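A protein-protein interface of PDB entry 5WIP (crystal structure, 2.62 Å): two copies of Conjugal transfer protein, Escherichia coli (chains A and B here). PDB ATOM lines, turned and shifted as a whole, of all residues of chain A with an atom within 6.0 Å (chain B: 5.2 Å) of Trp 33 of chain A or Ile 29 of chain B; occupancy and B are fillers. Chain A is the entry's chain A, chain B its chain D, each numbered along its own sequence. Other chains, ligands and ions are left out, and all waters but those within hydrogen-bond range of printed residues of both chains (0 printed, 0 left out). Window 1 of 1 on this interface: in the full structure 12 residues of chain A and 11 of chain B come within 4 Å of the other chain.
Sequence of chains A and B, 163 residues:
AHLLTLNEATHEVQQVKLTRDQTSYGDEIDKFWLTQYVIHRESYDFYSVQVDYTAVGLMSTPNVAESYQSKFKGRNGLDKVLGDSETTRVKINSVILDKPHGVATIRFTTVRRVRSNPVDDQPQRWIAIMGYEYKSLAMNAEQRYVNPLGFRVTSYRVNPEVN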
ATOM      1  N   GLU A  28     -10.665  35.371  10.247  1.00  0.00           N
ATOM      2  CA  GLU A  28     -11.743  34.979  11.149  1.00  0.00           C
ATOM      3  C   GLU A  28     -12.301  33.601  10.816  1.00  0.00           C
ATOM      4  O   GLU A  28     -12.820  32.916  11.704  1.00  0.00           O
ATOM      5  CB  GLU A  28     -12.852  36.028  11.123  1.00  0.00           C
ATOM      6  CG  GLU A  28     -12.387  37.401  11.573  1.00  0.00           C
ATOM      7  CD  GLU A  28     -11.775  37.379  12.962  1.00  0.00           C
ATOM      8  OE1 GLU A  28     -12.450  36.917  13.905  1.00  0.00           O
ATOM      9  OE2 GLU A  28     -10.615  37.816  13.110  1.00  0.00           O
ATOM     10  N   ILE A  29     -12.211  33.180   9.555  1.00  0.00           N
ATOM     11  CA  ILE A  29     -12.712  31.862   9.181  1.00  0.00           C
ATOM     12  C   ILE A  29     -11.708  30.781   9.556  1.00  0.00           C
ATOM     13  O   ILE A  29     -12.070  29.752  10.140  1.00  0.00           O
ATOM     14  CB  ILE A  29     -13.055  31.823   7.681  1.00  0.00           C
ATOM     15  CG1 ILE A  29     -14.127  32.865   7.359  1.00  0.00           C
ATOM     16  CG2 ILE A  29     -13.524  30.435   7.280  1.00  0.00           C
ATOM     17  CD1 ILE A  29     -14.487  32.939   5.893  1.00  0.00           C
ATOM     18  N   ASP A  30     -10.431  30.995   9.229  1.00  0.00           N
ATOM     19  CA  ASP A  30      -9.394  30.067   9.668  1.00  0.00           C
ATOM     20  C   ASP A  30      -9.375  29.950  11.187  1.00  0.00           C
ATOM     21  O   ASP A  30      -9.288  28.844  11.732  1.00  0.00           O
ATOM     22  CB  ASP A  30      -8.028  30.516   9.149  1.00  0.00           C
ATOM     23  CG  ASP A  30      -7.919  30.435   7.640  1.00  0.00           C
ATOM     24  OD1 ASP A  30      -8.856  29.913   7.000  1.00  0.00           O
ATOM     25  OD2 ASP A  30      -6.895  30.896   7.092  1.00  0.00           O
ATOM     26  N   LYS A  31      -9.464  31.085  11.886  1.00  0.00           N
ATOM     27  CA  LYS A  31      -9.440  31.063  13.345  1.00  0.00           C
ATOM     28  C   LYS A  31     -10.593  30.250  13.917  1.00  0.00           C
ATOM     29  O   LYS A  31     -10.457  29.654  14.991  1.00  0.00           O
ATOM     30  CB  LYS A  31      -9.477  32.490  13.893  1.00  0.00           C
ATOM     31  CG  LYS A  31      -9.505  32.559  15.410  1.00  0.00           C
ATOM     32  CD  LYS A  31      -9.767  33.971  15.902  1.00  0.00           C
ATOM     33  CE  LYS A  31      -9.916  34.004  17.413  1.00  0.00           C
ATOM     34  NZ  LYS A  31     -10.288  35.359  17.899  1.00  0.00           N
ATOM     35  N   PHE A  32     -11.734  30.216  13.226  1.00  0.00           N
ATOM     36  CA  PHE A  32     -12.877  29.464  13.735  1.00  0.00           C
ATOM     37  C   PHE A  32     -12.600  27.966  13.725  1.00  0.00           C
ATOM     38  O   PHE A  32     -12.773  27.286  14.743  1.00  0.00           O
ATOM     39  CB  PHE A  32     -14.127  29.777  12.915  1.00  0.00           C
ATOM     40  CG  PHE A  32     -15.282  28.862  13.207  1.00  0.00           C
ATOM     41  CD1 PHE A  32     -16.009  28.998  14.375  1.00  0.00           C
ATOM     42  CD2 PHE A  32     -15.631  27.857  12.318  1.00  0.00           C
ATOM     43  CE1 PHE A  32     -17.069  28.155  14.652  1.00  0.00           C
ATOM     44  CE2 PHE A  32     -16.691  27.011  12.589  1.00  0.00           C
ATOM     45  CZ  PHE A  32     -17.411  27.160  13.758  1.00  0.00           C
ATOM     46  N   TRP A  33     -12.172  27.433  12.579  1.00  0.00           N
ATOM     47  CA  TRP A  33     -11.944  25.996  12.471  1.00  0.00           C
ATOM     48  C   TRP A  33     -10.757  25.556  13.319  1.00  0.00           C
ATOM     49  O   TRP A  33     -10.810  24.508  13.973  1.00  0.00           O
ATOM     50  CB  TRP A  33     -11.734  25.607  11.008  1.00  0.00           C
ATOM     51  CG  TRP A  33     -12.902  25.940  10.131  1.00  0.00           C
ATOM     52  CD1 TRP A  33     -12.968  26.929   9.192  1.00  0.00           C
ATOM     53  CD2 TRP A  33     -14.179  25.291  10.120  1.00  0.00           C
ATOM     54  NE1 TRP A  33     -14.206  26.931   8.593  1.00  0.00           N
ATOM     55  CE2 TRP A  33     -14.967  25.935   9.145  1.00  0.00           C
ATOM     56  CE3 TRP A  33     -14.733  24.226  10.838  1.00  0.00           C
ATOM     57  CZ2 TRP A  33     -16.279  25.550   8.870  1.00  0.00           C
ATOM     58  CZ3 TRP A  33     -16.035  23.844  10.563  1.00  0.00           C
ATOM     59  CH2 TRP A  33     -16.792  24.505   9.588  1.00  0.00           C
ATOM     60  N   LEU A  34      -9.678  26.342  13.320  1.00  0.00           N
ATOM     61  CA  LEU A  34      -8.502  25.980  14.103  1.00  0.00           C
ATOM     62  C   LEU A  34      -8.845  25.861  15.583  1.00  0.00           C
ATOM     63  O   LEU A  34      -8.479  24.880  16.242  1.00  0.00           O
ATOM     64  CB  LEU A  34      -7.392  27.006  13.882  1.00  0.00           C
ATOM     65  CG  LEU A  34      -6.775  27.030  12.481  1.00  0.00           C
ATOM     66  CD1 LEU A  34      -6.002  28.320  12.267  1.00  0.00           C
ATOM     67  CD2 LEU A  34      -5.874  25.821  12.275  1.00  0.00           C
ATOM     68  N   THR A  35      -9.552  26.856  16.125  1.00  0.00           N
ATOM     69  CA  THR A  35      -9.955  26.790  17.526  1.00  0.00           C
ATOM     70  C   THR A  35     -10.992  25.696  17.750  1.00  0.00           C
ATOM     71  O   THR A  35     -10.988  25.033  18.793  1.00  0.00           O
ATOM     72  CB  THR A  35     -10.495  28.146  17.986  1.00  0.00           C
ATOM     73  OG1 THR A  35     -11.658  28.486  17.221  1.00  0.00           O
ATOM     74  CG2 THR A  35      -9.441  29.226  17.803  1.00  0.00           C
ATOM     75  N   GLN A  36     -11.889  25.494  16.782  1.00  0.00           N
ATOM     76  CA  GLN A  36     -12.846  24.397  16.884  1.00  0.00           C
ATOM     77  C   GLN A  36     -12.132  23.053  16.942  1.00  0.00           C
ATOM     78  O   GLN A  36     -12.524  22.163  17.706  1.00  0.00           O
ATOM     79  CB  GLN A  36     -13.821  24.438  15.707  1.00  0.00           C
ATOM     80  CG  GLN A  36     -14.921  25.476  15.854  1.00  0.00           C
ATOM     81  CD  GLN A  36     -15.826  25.194  17.037  1.00  0.00           C
ATOM     82  OE1 GLN A  36     -15.847  25.946  18.011  1.00  0.00           O
ATOM     83  NE2 GLN A  36     -16.581  24.103  16.958  1.00  0.00           N
ATOM     84  N   TYR A  37     -11.078  22.890  16.142  1.00  0.00           N
ATOM     85  CA  TYR A  37     -10.320  21.644  16.151  1.00  0.00           C
ATOM     86  C   TYR A  37      -9.672  21.411  17.511  1.00  0.00           C
ATOM     87  O   TYR A  37      -9.738  20.306  18.063  1.00  0.00           O
ATOM     88  CB  TYR A  37      -9.265  21.676  15.046  1.00  0.00           C
ATOM     89  CG  TYR A  37      -8.538  20.370  14.834  1.00  0.00           C
ATOM     90  CD1 TYR A  37      -7.384  20.069  15.546  1.00  0.00           C
ATOM     91  CD2 TYR A  37      -8.997  19.440  13.913  1.00  0.00           C
ATOM     92  CE1 TYR A  37      -6.714  18.875  15.351  1.00  0.00           C
ATOM     93  CE2 TYR A  37      -8.334  18.246  13.710  1.00  0.00           C
ATOM     94  CZ  TYR A  37      -7.194  17.967  14.432  1.00  0.00           C
ATOM     95  OH  TYR A  37      -6.533  16.776  14.228  1.00  0.00           O
ATOM     96  N   VAL A  38      -9.044  22.449  18.068  1.00  0.00           N
ATOM     97  CA  VAL A  38      -8.360  22.303  19.350  1.00  0.00           C
ATOM     98  C   VAL A  38      -9.355  21.994  20.461  1.00  0.00           C
ATOM     99  O   VAL A  38      -9.057  21.226  21.383  1.00  0.00           O
ATOM    100  CB  VAL A  38      -7.538  23.565  19.665  1.00  0.00           C
ATOM    101  CG1 VAL A  38      -7.054  23.538  21.111  1.00  0.00           C
ATOM    102  CG2 VAL A  38      -6.363  23.684  18.707  1.00  0.00           C
ATOM    103  N   MET A  59     -11.728  16.404  10.259  1.00  0.00           N
ATOM    104  CA  MET A  59     -10.961  17.589  10.105  1.00  0.00           C
ATOM    105  C   MET A  59      -9.491  17.352  10.081  1.00  0.00           C
ATOM    106  O   MET A  59      -8.736  18.192  10.278  1.00  0.00           O
ATOM    107  CB  MET A  59     -11.353  18.594  11.146  1.00  0.00           C
ATOM    108  CG  MET A  59     -12.814  18.733  11.364  1.00  0.00           C
ATOM    109  SD  MET A  59     -13.349  20.165  12.233  1.00  0.00           S
ATOM    110  CE  MET A  59     -12.635  19.926  13.762  1.00  0.00           C
ATOM    111  N   MET A 130       0.163  23.968  14.568  1.00  0.00           N
ATOM    112  CA  MET A 130      -0.720  23.271  13.649  1.00  0.00           C
ATOM    113  C   MET A 130      -0.426  23.676  12.213  1.00  0.00           C
ATOM    114  O   MET A 130       0.032  24.788  11.943  1.00  0.00           O
ATOM    115  CB  MET A 130      -2.189  23.568  13.968  1.00  0.00           C
ATOM    116  CG  MET A 130      -2.532  23.485  15.444  1.00  0.00           C
ATOM    117  SD  MET A 130      -4.127  24.241  15.805  1.00  0.00           S
ATOM    118  CE  MET A 130      -5.199  23.273  14.747  1.00  0.00           C
ATOM    119  N   TYR A 134      -7.518  23.548   3.158  1.00  0.00           N
ATOM    120  CA  TYR A 134      -8.884  23.211   2.781  1.00  0.00           C
ATOM    121  C   TYR A 134      -8.849  22.373   1.513  1.00  0.00           C
ATOM    122  O   TYR A 134      -8.100  22.678   0.580  1.00  0.00           O
ATOM    123  CB  TYR A 134      -9.740  24.466   2.561  1.00  0.00           C
ATOM    124  CG  TYR A 134      -9.930  25.313   3.800  1.00  0.00           C
ATOM    125  CD1 TYR A 134      -8.966  26.233   4.190  1.00  0.00           C
ATOM    126  CD2 TYR A 134     -11.076  25.198   4.577  1.00  0.00           C
ATOM    127  CE1 TYR A 134      -9.136  27.011   5.319  1.00  0.00           C
ATOM    128  CE2 TYR A 134     -11.255  25.973   5.708  1.00  0.00           C
ATOM    129  CZ  TYR A 134     -10.280  26.878   6.074  1.00  0.00           C
ATOM    130  OH  TYR A 134     -10.445  27.655   7.198  1.00  0.00           O
ATOM    131  N   ARG A 144     -20.783  16.954   5.439  1.00  0.00           N
ATOM    132  CA  ARG A 144     -20.848  18.373   5.100  1.00  0.00           C
ATOM    133  C   ARG A 144     -21.496  19.185   6.214  1.00  0.00           C
ATOM    134  O   ARG A 144     -21.150  20.356   6.408  1.00  0.00           O
ATOM    135  CB  ARG A 144     -21.608  18.572   3.788  1.00  0.00           C
ATOM    136  CG  ARG A 144     -20.801  18.241   2.544  1.00  0.00           C
ATOM    137  CD  ARG A 144     -21.564  18.585   1.274  1.00  0.00           C
ATOM    138  NE  ARG A 144     -22.730  17.728   1.082  1.00  0.00           N
ATOM    139  CZ  ARG A 144     -23.951  18.013   1.524  1.00  0.00           C
ATOM    140  NH1 ARG A 144     -24.174  19.140   2.187  1.00  0.00           N
ATOM    141  NH2 ARG A 144     -24.952  17.172   1.301  1.00  0.00           N
ATOM    142  N   TYR A 145     -22.431  18.583   6.949  1.00  0.00           N
ATOM    143  CA  TYR A 145     -23.046  19.252   8.089  1.00  0.00           C
ATOM    144  C   TYR A 145     -22.028  19.599   9.168  1.00  0.00           C
ATOM    145  O   TYR A 145     -22.309  20.451  10.018  1.00  0.00           O
ATOM    146  CB  TYR A 145     -24.151  18.359   8.662  1.00  0.00           C
ATOM    147  CG  TYR A 145     -24.901  18.932   9.845  1.00  0.00           C
ATOM    148  CD1 TYR A 145     -26.054  19.683   9.662  1.00  0.00           C
ATOM    149  CD2 TYR A 145     -24.471  18.702  11.145  1.00  0.00           C
ATOM    150  CE1 TYR A 145     -26.750  20.201  10.741  1.00  0.00           C
ATOM    151  CE2 TYR A 145     -25.160  19.216  12.230  1.00  0.00           C
ATOM    152  CZ  TYR A 145     -26.299  19.964  12.022  1.00  0.00           C
ATOM    153  OH  TYR A 145     -26.990  20.479  13.096  1.00  0.00           O
ATOM    154  N   VAL A 146     -20.854  18.968   9.149  1.00  0.00           N
ATOM    155  CA  VAL A 146     -19.849  19.178  10.176  1.00  0.00           C
ATOM    156  C   VAL A 146     -18.592  19.859   9.642  1.00  0.00           C
ATOM    157  O   VAL A 146     -17.948  20.608  10.386  1.00  0.00           O
ATOM    158  CB  VAL A 146     -19.491  17.846  10.866  1.00  0.00           C
ATOM    159  CG1 VAL A 146     -18.302  18.031  11.794  1.00  0.00           C
ATOM    160  CG2 VAL A 146     -20.688  17.303  11.629  1.00  0.00           C
ATOM    161  N   ASN A 147     -18.219  19.622   8.385  1.00  0.00           N
ATOM    162  CA  ASN A 147     -17.011  20.200   7.797  1.00  0.00           C
ATOM    163  C   ASN A 147     -17.338  20.727   6.403  1.00  0.00           C
ATOM    164  O   ASN A 147     -16.784  20.272   5.399  1.00  0.00           O
ATOM    165  CB  ASN A 147     -15.885  19.167   7.753  1.00  0.00           C
ATOM    166  CG  ASN A 147     -14.510  19.796   7.856  1.00  0.00           C
ATOM    167  OD1 ASN A 147     -14.344  20.870   8.434  1.00  0.00           O
ATOM    168  ND2 ASN A 147     -13.511  19.123   7.294  1.00  0.00           N
ATOM    169  N   PRO A 148     -18.241  21.707   6.313  1.00  0.00           N
ATOM    170  CA  PRO A 148     -18.708  22.161   4.990  1.00  0.00           C
ATOM    171  C   PRO A 148     -17.589  22.598   4.058  1.00  0.00           C
ATOM    172  O   PRO A 148     -17.611  22.257   2.868  1.00  0.00           O
ATOM    173  CB  PRO A 148     -19.642  23.329   5.338  1.00  0.00           C
ATOM    174  CG  PRO A 148     -20.059  23.082   6.754  1.00  0.00           C
ATOM    175  CD  PRO A 148     -18.876  22.449   7.414  1.00  0.00           C
ATOM    176  N   LEU A 149     -16.611  23.343   4.564  1.00  0.00           N
ATOM    177  CA  LEU A 149     -15.541  23.886   3.741  1.00  0.00           C
ATOM    178  C   LEU A 149     -14.370  22.927   3.567  1.00  0.00           C
ATOM    179  O   LEU A 149     -13.375  23.297   2.936  1.00  0.00           O
ATOM    180  CB  LEU A 149     -15.037  25.205   4.337  1.00  0.00           C
ATOM    181  CG  LEU A 149     -16.095  26.277   4.608  1.00  0.00           C
ATOM    182  CD1 LEU A 149     -15.440  27.589   5.018  1.00  0.00           C
ATOM    183  CD2 LEU A 149     -16.992  26.469   3.394  1.00  0.00           C
ATOM    184  N   PHE A 151     -12.218  21.728   5.851  1.00  0.00           N
ATOM    185  CA  PHE A 151     -11.047  22.046   6.656  1.00  0.00           C
ATOM    186  C   PHE A 151     -10.428  20.770   7.213  1.00  0.00           C
ATOM    187  O   PHE A 151     -11.131  19.802   7.522  1.00  0.00           O
ATOM    188  CB  PHE A 151     -11.439  22.990   7.798  1.00  0.00           C
ATOM    189  CG  PHE A 151     -10.313  23.312   8.742  1.00  0.00           C
ATOM    190  CD1 PHE A 151     -10.069  22.512   9.847  1.00  0.00           C
ATOM    191  CD2 PHE A 151      -9.509  24.420   8.535  1.00  0.00           C
ATOM    192  CE1 PHE A 151      -9.039  22.805  10.719  1.00  0.00           C
ATOM    193  CE2 PHE A 151      -8.477  24.719   9.406  1.00  0.00           C
ATOM    194  CZ  PHE A 151      -8.243  23.911  10.499  1.00  0.00           C
ATOM    195  N   TYR B  25     -26.150  23.394   9.270  1.00  0.00           N
ATOM    196  CA  TYR B  25     -24.743  23.202   9.381  1.00  0.00           C
ATOM    197  C   TYR B  25     -24.217  22.961  10.791  1.00  0.00           C
ATOM    198  O   TYR B  25     -23.066  22.660  10.956  1.00  0.00           O
ATOM    199  CB  TYR B  25     -24.073  24.384   8.769  1.00  0.00           C
ATOM    200  CG  TYR B  25     -23.976  24.359   7.293  1.00  0.00           C
ATOM    201  CD1 TYR B  25     -23.337  23.357   6.644  1.00  0.00           C
ATOM    202  CD2 TYR B  25     -24.469  25.374   6.542  1.00  0.00           C
ATOM    203  CE1 TYR B  25     -23.231  23.348   5.282  1.00  0.00           C
ATOM    204  CE2 TYR B  25     -24.368  25.360   5.184  1.00  0.00           C
ATOM    205  CZ  TYR B  25     -23.750  24.337   4.572  1.00  0.00           C
ATOM    206  OH  TYR B  25     -23.642  24.324   3.242  1.00  0.00           O
ATOM    207  N   GLY B  26     -25.024  23.085  11.816  1.00  0.00           N
ATOM    208  CA  GLY B  26     -24.566  22.878  13.178  1.00  0.00           C
ATOM    209  C   GLY B  26     -24.626  24.126  14.043  1.00  0.00           C
ATOM    210  O   GLY B  26     -24.562  25.243  13.525  1.00  0.00           O
ATOM    211  N   ASP B  27     -24.736  23.958  15.365  1.00  0.00           N
ATOM    212  CA  ASP B  27     -24.923  25.109  16.250  1.00  0.00           C
ATOM    213  C   ASP B  27     -23.714  26.040  16.236  1.00  0.00           C
ATOM    214  O   ASP B  27     -23.861  27.259  16.089  1.00  0.00           O
ATOM    215  CB  ASP B  27     -25.209  24.637  17.677  1.00  0.00           C
ATOM    216  CG  ASP B  27     -26.624  24.118  17.854  1.00  0.00           C
ATOM    217  OD1 ASP B  27     -27.054  23.276  17.037  1.00  0.00           O
ATOM    218  OD2 ASP B  27     -27.300  24.543  18.814  1.00  0.00           O
ATOM    219  N   GLU B  28     -22.507  25.490  16.404  1.00  0.00           N
ATOM    220  CA  GLU B  28     -21.320  26.338  16.476  1.00  0.00           C
ATOM    221  C   GLU B  28     -21.048  27.054  15.159  1.00  0.00           C
ATOM    222  O   GLU B  28     -20.508  28.165  15.163  1.00  0.00           O
ATOM    223  CB  GLU B  28     -20.107  25.512  16.903  1.00  0.00           C
ATOM    224  CG  GLU B  28     -20.242  24.954  18.307  1.00  0.00           C
ATOM    225  CD  GLU B  28     -20.634  26.024  19.312  1.00  0.00           C
ATOM    226  OE1 GLU B  28     -20.007  27.104  19.310  1.00  0.00           O
ATOM    227  OE2 GLU B  28     -21.580  25.792  20.096  1.00  0.00           O
ATOM    228  N   ILE B  29     -21.406  26.442  14.030  1.00  0.00           N
ATOM    229  CA  ILE B  29     -21.268  27.133  12.752  1.00  0.00           C
ATOM    230  C   ILE B  29     -22.282  28.264  12.649  1.00  0.00           C
ATOM    231  O   ILE B  29     -21.988  29.335  12.105  1.00  0.00           O
ATOM    232  CB  ILE B  29     -21.406  26.140  11.585  1.00  0.00           C
ATOM    233  CG1 ILE B  29     -20.316  25.070  11.660  1.00  0.00           C
ATOM    234  CG2 ILE B  29     -21.340  26.874  10.254  1.00  0.00           C
ATOM    235  CD1 ILE B  29     -20.392  24.043  10.550  1.00  0.00           C
ATOM    236  N   ASP B  30     -23.491  28.048  13.173  1.00  0.00           N
ATOM    237  CA  ASP B  30     -24.501  29.101  13.169  1.00  0.00           C
ATOM    238  C   ASP B  30     -24.065  30.283  14.025  1.00  0.00           C
ATOM    239  O   ASP B  30     -24.170  31.442  13.607  1.00  0.00           O
ATOM    240  CB  ASP B  30     -25.837  28.545  13.661  1.00  0.00           C
ATOM    241  CG  ASP B  30     -26.537  27.705  12.615  1.00  0.00           C
ATOM    242  OD1 ASP B  30     -26.058  27.675  11.463  1.00  0.00           O
ATOM    243  OD2 ASP B  30     -27.565  27.078  12.943  1.00  0.00           O
ATOM    244  N   LYS B  31     -23.570  30.005  15.233  1.00  0.00           N
ATOM    245  CA  LYS B  31     -23.165  31.072  16.141  1.00  0.00           C
ATOM    246  C   LYS B  31     -21.992  31.883  15.606  1.00  0.00           C
ATOM    247  O   LYS B  31     -21.825  33.042  16.001  1.00  0.00           O
ATOM    248  CB  LYS B  31     -22.809  30.491  17.509  1.00  0.00           C
ATOM    249  CG  LYS B  31     -23.935  29.717  18.170  1.00  0.00           C
ATOM    250  CD  LYS B  31     -23.528  29.236  19.553  1.00  0.00           C
ATOM    251  CE  LYS B  31     -24.649  28.458  20.219  1.00  0.00           C
ATOM    252  NZ  LYS B  31     -24.292  28.039  21.601  1.00  0.00           N
ATOM    253  N   PHE B  32     -21.174  31.306  14.725  1.00  0.00           N
ATOM    254  CA  PHE B  32     -20.041  32.045  14.179  1.00  0.00           C
ATOM    255  C   PHE B  32     -20.508  33.134  13.221  1.00  0.00           C
ATOM    256  O   PHE B  32     -20.133  34.303  13.363  1.00  0.00           O
ATOM    257  CB  PHE B  32     -19.074  31.091  13.479  1.00  0.00           C
ATOM    258  CG  PHE B  32     -17.958  31.789  12.755  1.00  0.00           C
ATOM    259  CD1 PHE B  32     -16.895  32.330  13.457  1.00  0.00           C
ATOM    260  CD2 PHE B  32     -17.972  31.902  11.374  1.00  0.00           C
ATOM    261  CE1 PHE B  32     -15.865  32.973  12.795  1.00  0.00           C
ATOM    262  CE2 PHE B  32     -16.945  32.544  10.707  1.00  0.00           C
ATOM    263  CZ  PHE B  32     -15.890  33.080  11.418  1.00  0.00           C
ATOM    264  N   TRP B  33     -21.331  32.766  12.237  1.00  0.00           N
ATOM    265  CA  TRP B  33     -21.816  33.748  11.274  1.00  0.00           C
ATOM    266  C   TRP B  33     -22.755  34.750  11.932  1.00  0.00           C
ATOM    267  O   TRP B  33     -22.750  35.936  11.583  1.00  0.00           O
ATOM    268  CB  TRP B  33     -22.507  33.038  10.111  1.00  0.00           C
ATOM    269  CG  TRP B  33     -21.615  32.071   9.394  1.00  0.00           C
ATOM    270  CD1 TRP B  33     -21.666  30.708   9.449  1.00  0.00           C
ATOM    271  CD2 TRP B  33     -20.527  32.396   8.522  1.00  0.00           C
ATOM    272  NE1 TRP B  33     -20.681  30.165   8.658  1.00  0.00           N
ATOM    273  CE2 TRP B  33     -19.968  31.182   8.079  1.00  0.00           C
ATOM    274  CE3 TRP B  33     -19.974  33.598   8.070  1.00  0.00           C
ATOM    275  CZ2 TRP B  33     -18.882  31.134   7.207  1.00  0.00           C
ATOM    276  CZ3 TRP B  33     -18.898  33.548   7.205  1.00  0.00           C
ATOM    277  CH2 TRP B  33     -18.363  32.326   6.782  1.00  0.00           C
ATOM    278  N   TYR B 134     -29.358  29.685   4.909  1.00  0.00           N
ATOM    279  CA  TYR B 134     -28.251  29.450   3.994  1.00  0.00           C
ATOM    280  C   TYR B 134     -28.790  29.201   2.594  1.00  0.00           C
ATOM    281  O   TYR B 134     -29.882  28.652   2.418  1.00  0.00           O
ATOM    282  CB  TYR B 134     -27.391  28.259   4.443  1.00  0.00           C
ATOM    283  CG  TYR B 134     -26.743  28.440   5.797  1.00  0.00           C
ATOM    284  CD1 TYR B 134     -27.448  28.184   6.966  1.00  0.00           C
ATOM    285  CD2 TYR B 134     -25.422  28.858   5.908  1.00  0.00           C
ATOM    286  CE1 TYR B 134     -26.859  28.344   8.207  1.00  0.00           C
ATOM    287  CE2 TYR B 134     -24.824  29.021   7.144  1.00  0.00           C
ATOM    288  CZ  TYR B 134     -25.547  28.762   8.290  1.00  0.00           C
ATOM    289  OH  TYR B 134     -24.957  28.923   9.522  1.00  0.00           O
ATOM    290  N   LEU B 149     -20.484  29.902   2.863  1.00  0.00           N
ATOM    291  CA  LEU B 149     -21.628  29.017   3.051  1.00  0.00           C
ATOM    292  C   LEU B 149     -22.957  29.659   2.672  1.00  0.00           C
ATOM    293  O   LEU B 149     -23.997  29.006   2.804  1.00  0.00           O
ATOM    294  CB  LEU B 149     -21.694  28.538   4.504  1.00  0.00           C
ATOM    295  CG  LEU B 149     -20.537  27.671   5.004  1.00  0.00           C
ATOM    296  CD1 LEU B 149     -20.859  27.080   6.372  1.00  0.00           C
ATOM    297  CD2 LEU B 149     -20.214  26.573   4.003  1.00  0.00           C
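The side-chain hydroxyl (OG1) of Thr 35 of chain A lies within hydrogen-bond range of the backbone carbonyl oxygen (O) of Phe 32 of chain A (3.0 Å).
OE2 of Glu 28 of chain B is in salt-bridge range of NZ of Lys 31 of chain B (3.8 Å).
Among the printed residues, merely in contact across the chains: Glu 28 of chain A with Phe 32 of chain B (3.1 Å), Leu 149 of chain A with Leu 149 of chain B (3.3 Å), Pro 148 of chain A with Tyr 25 of chain B (3.3 Å), Tyr 145 of chain A with Gly 26 of chain B (3.4 Å), Phe 32 of chain A with Glu 28 of chain B (3.5 Å), Pro 148 of chain A with Leu 149 of chain B (3.6 Å), Phe 32 of chain A with Phe 32 of chain B (3.6 Å), Arg 144 of chain A with Tyr 25 of chain B (3.7 Å), Trp 33 of chain A with Ile 29 of chain B (3.8 Å), Gln 36 of chain A with Glu 28 of chain B (3.8 Å), Pro 148 of chain A with Ile 29 of chain B (3.8 Å) and Phe 32 of chain A with Ile 29 of chain B (3.99 Å).
Of chain B, only Ile 29 (3.8 Å) comes within 4 Å of Trp 33 of chain A.
Of the printed residues of chain B, Gln 36 of chain A touches Glu 28.
Printed residues of chain B within 4 Å of Pro 148 of chain A: Tyr 25, Ile 29 and Leu 149.
Printed residues of chain A within 4 Å of Gly 26 of chain B: Tyr 145.
Of the printed residues of chain A, Ile 29 of chain B touches Phe 32 (3.99 Å), Trp 33 (3.8 Å) and Pro 148 (3.8 Å).
The nearest printed residue of chain B that does not touch Trp 33 of chain A is Leu 149 of chain B (5.4 Å).
The nearest printed residue of chain B that does not touch Phe 32 of chain A is Asp 30 of chain B (6.2 Å).
Glu 28 of chain A touches Phe 32 of chain B, and with the chains exchanged Phe 32 of chain A touches Glu 28 of chain B.
Phe 32 of chain A touches Ile 29 of chain B, but with the chains exchanged Ile 29 of chain A does not touch Phe 32 of chain B (4.1 Å).
Phe 32 of chain A touches its own counterpart, Phe 32 of chain B.
Leu 149 of chain B touches its own counterpart, Leu 149 of chain A.
8 positions are printed for both chains.
Printed residues of chain B that touch a printed residue of chain A: Tyr 25, Gly 26, Glu 28, Ile 29, Phe 32 and Leu 149.
Printed residues of chain A that touch a printed residue of chain B: Glu 28, Phe 32, Trp 33, Gln 36, Arg 144, Tyr 145, Pro 148 and Leu 149.
Along chain A the printed residues that touch a printed residue of chain B span positions 28 to 149.
Among the printed residues, no Asp or Glu carboxylate lies within 4 Å of a Lys or Arg side-chain nitrogen of the other chain.
The backbone carbonyl oxygen (O) of Tyr 145 of chain A sits close to the backbone carbonyl oxygen (O) of Tyr 25 of chain B (2.5 Å).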
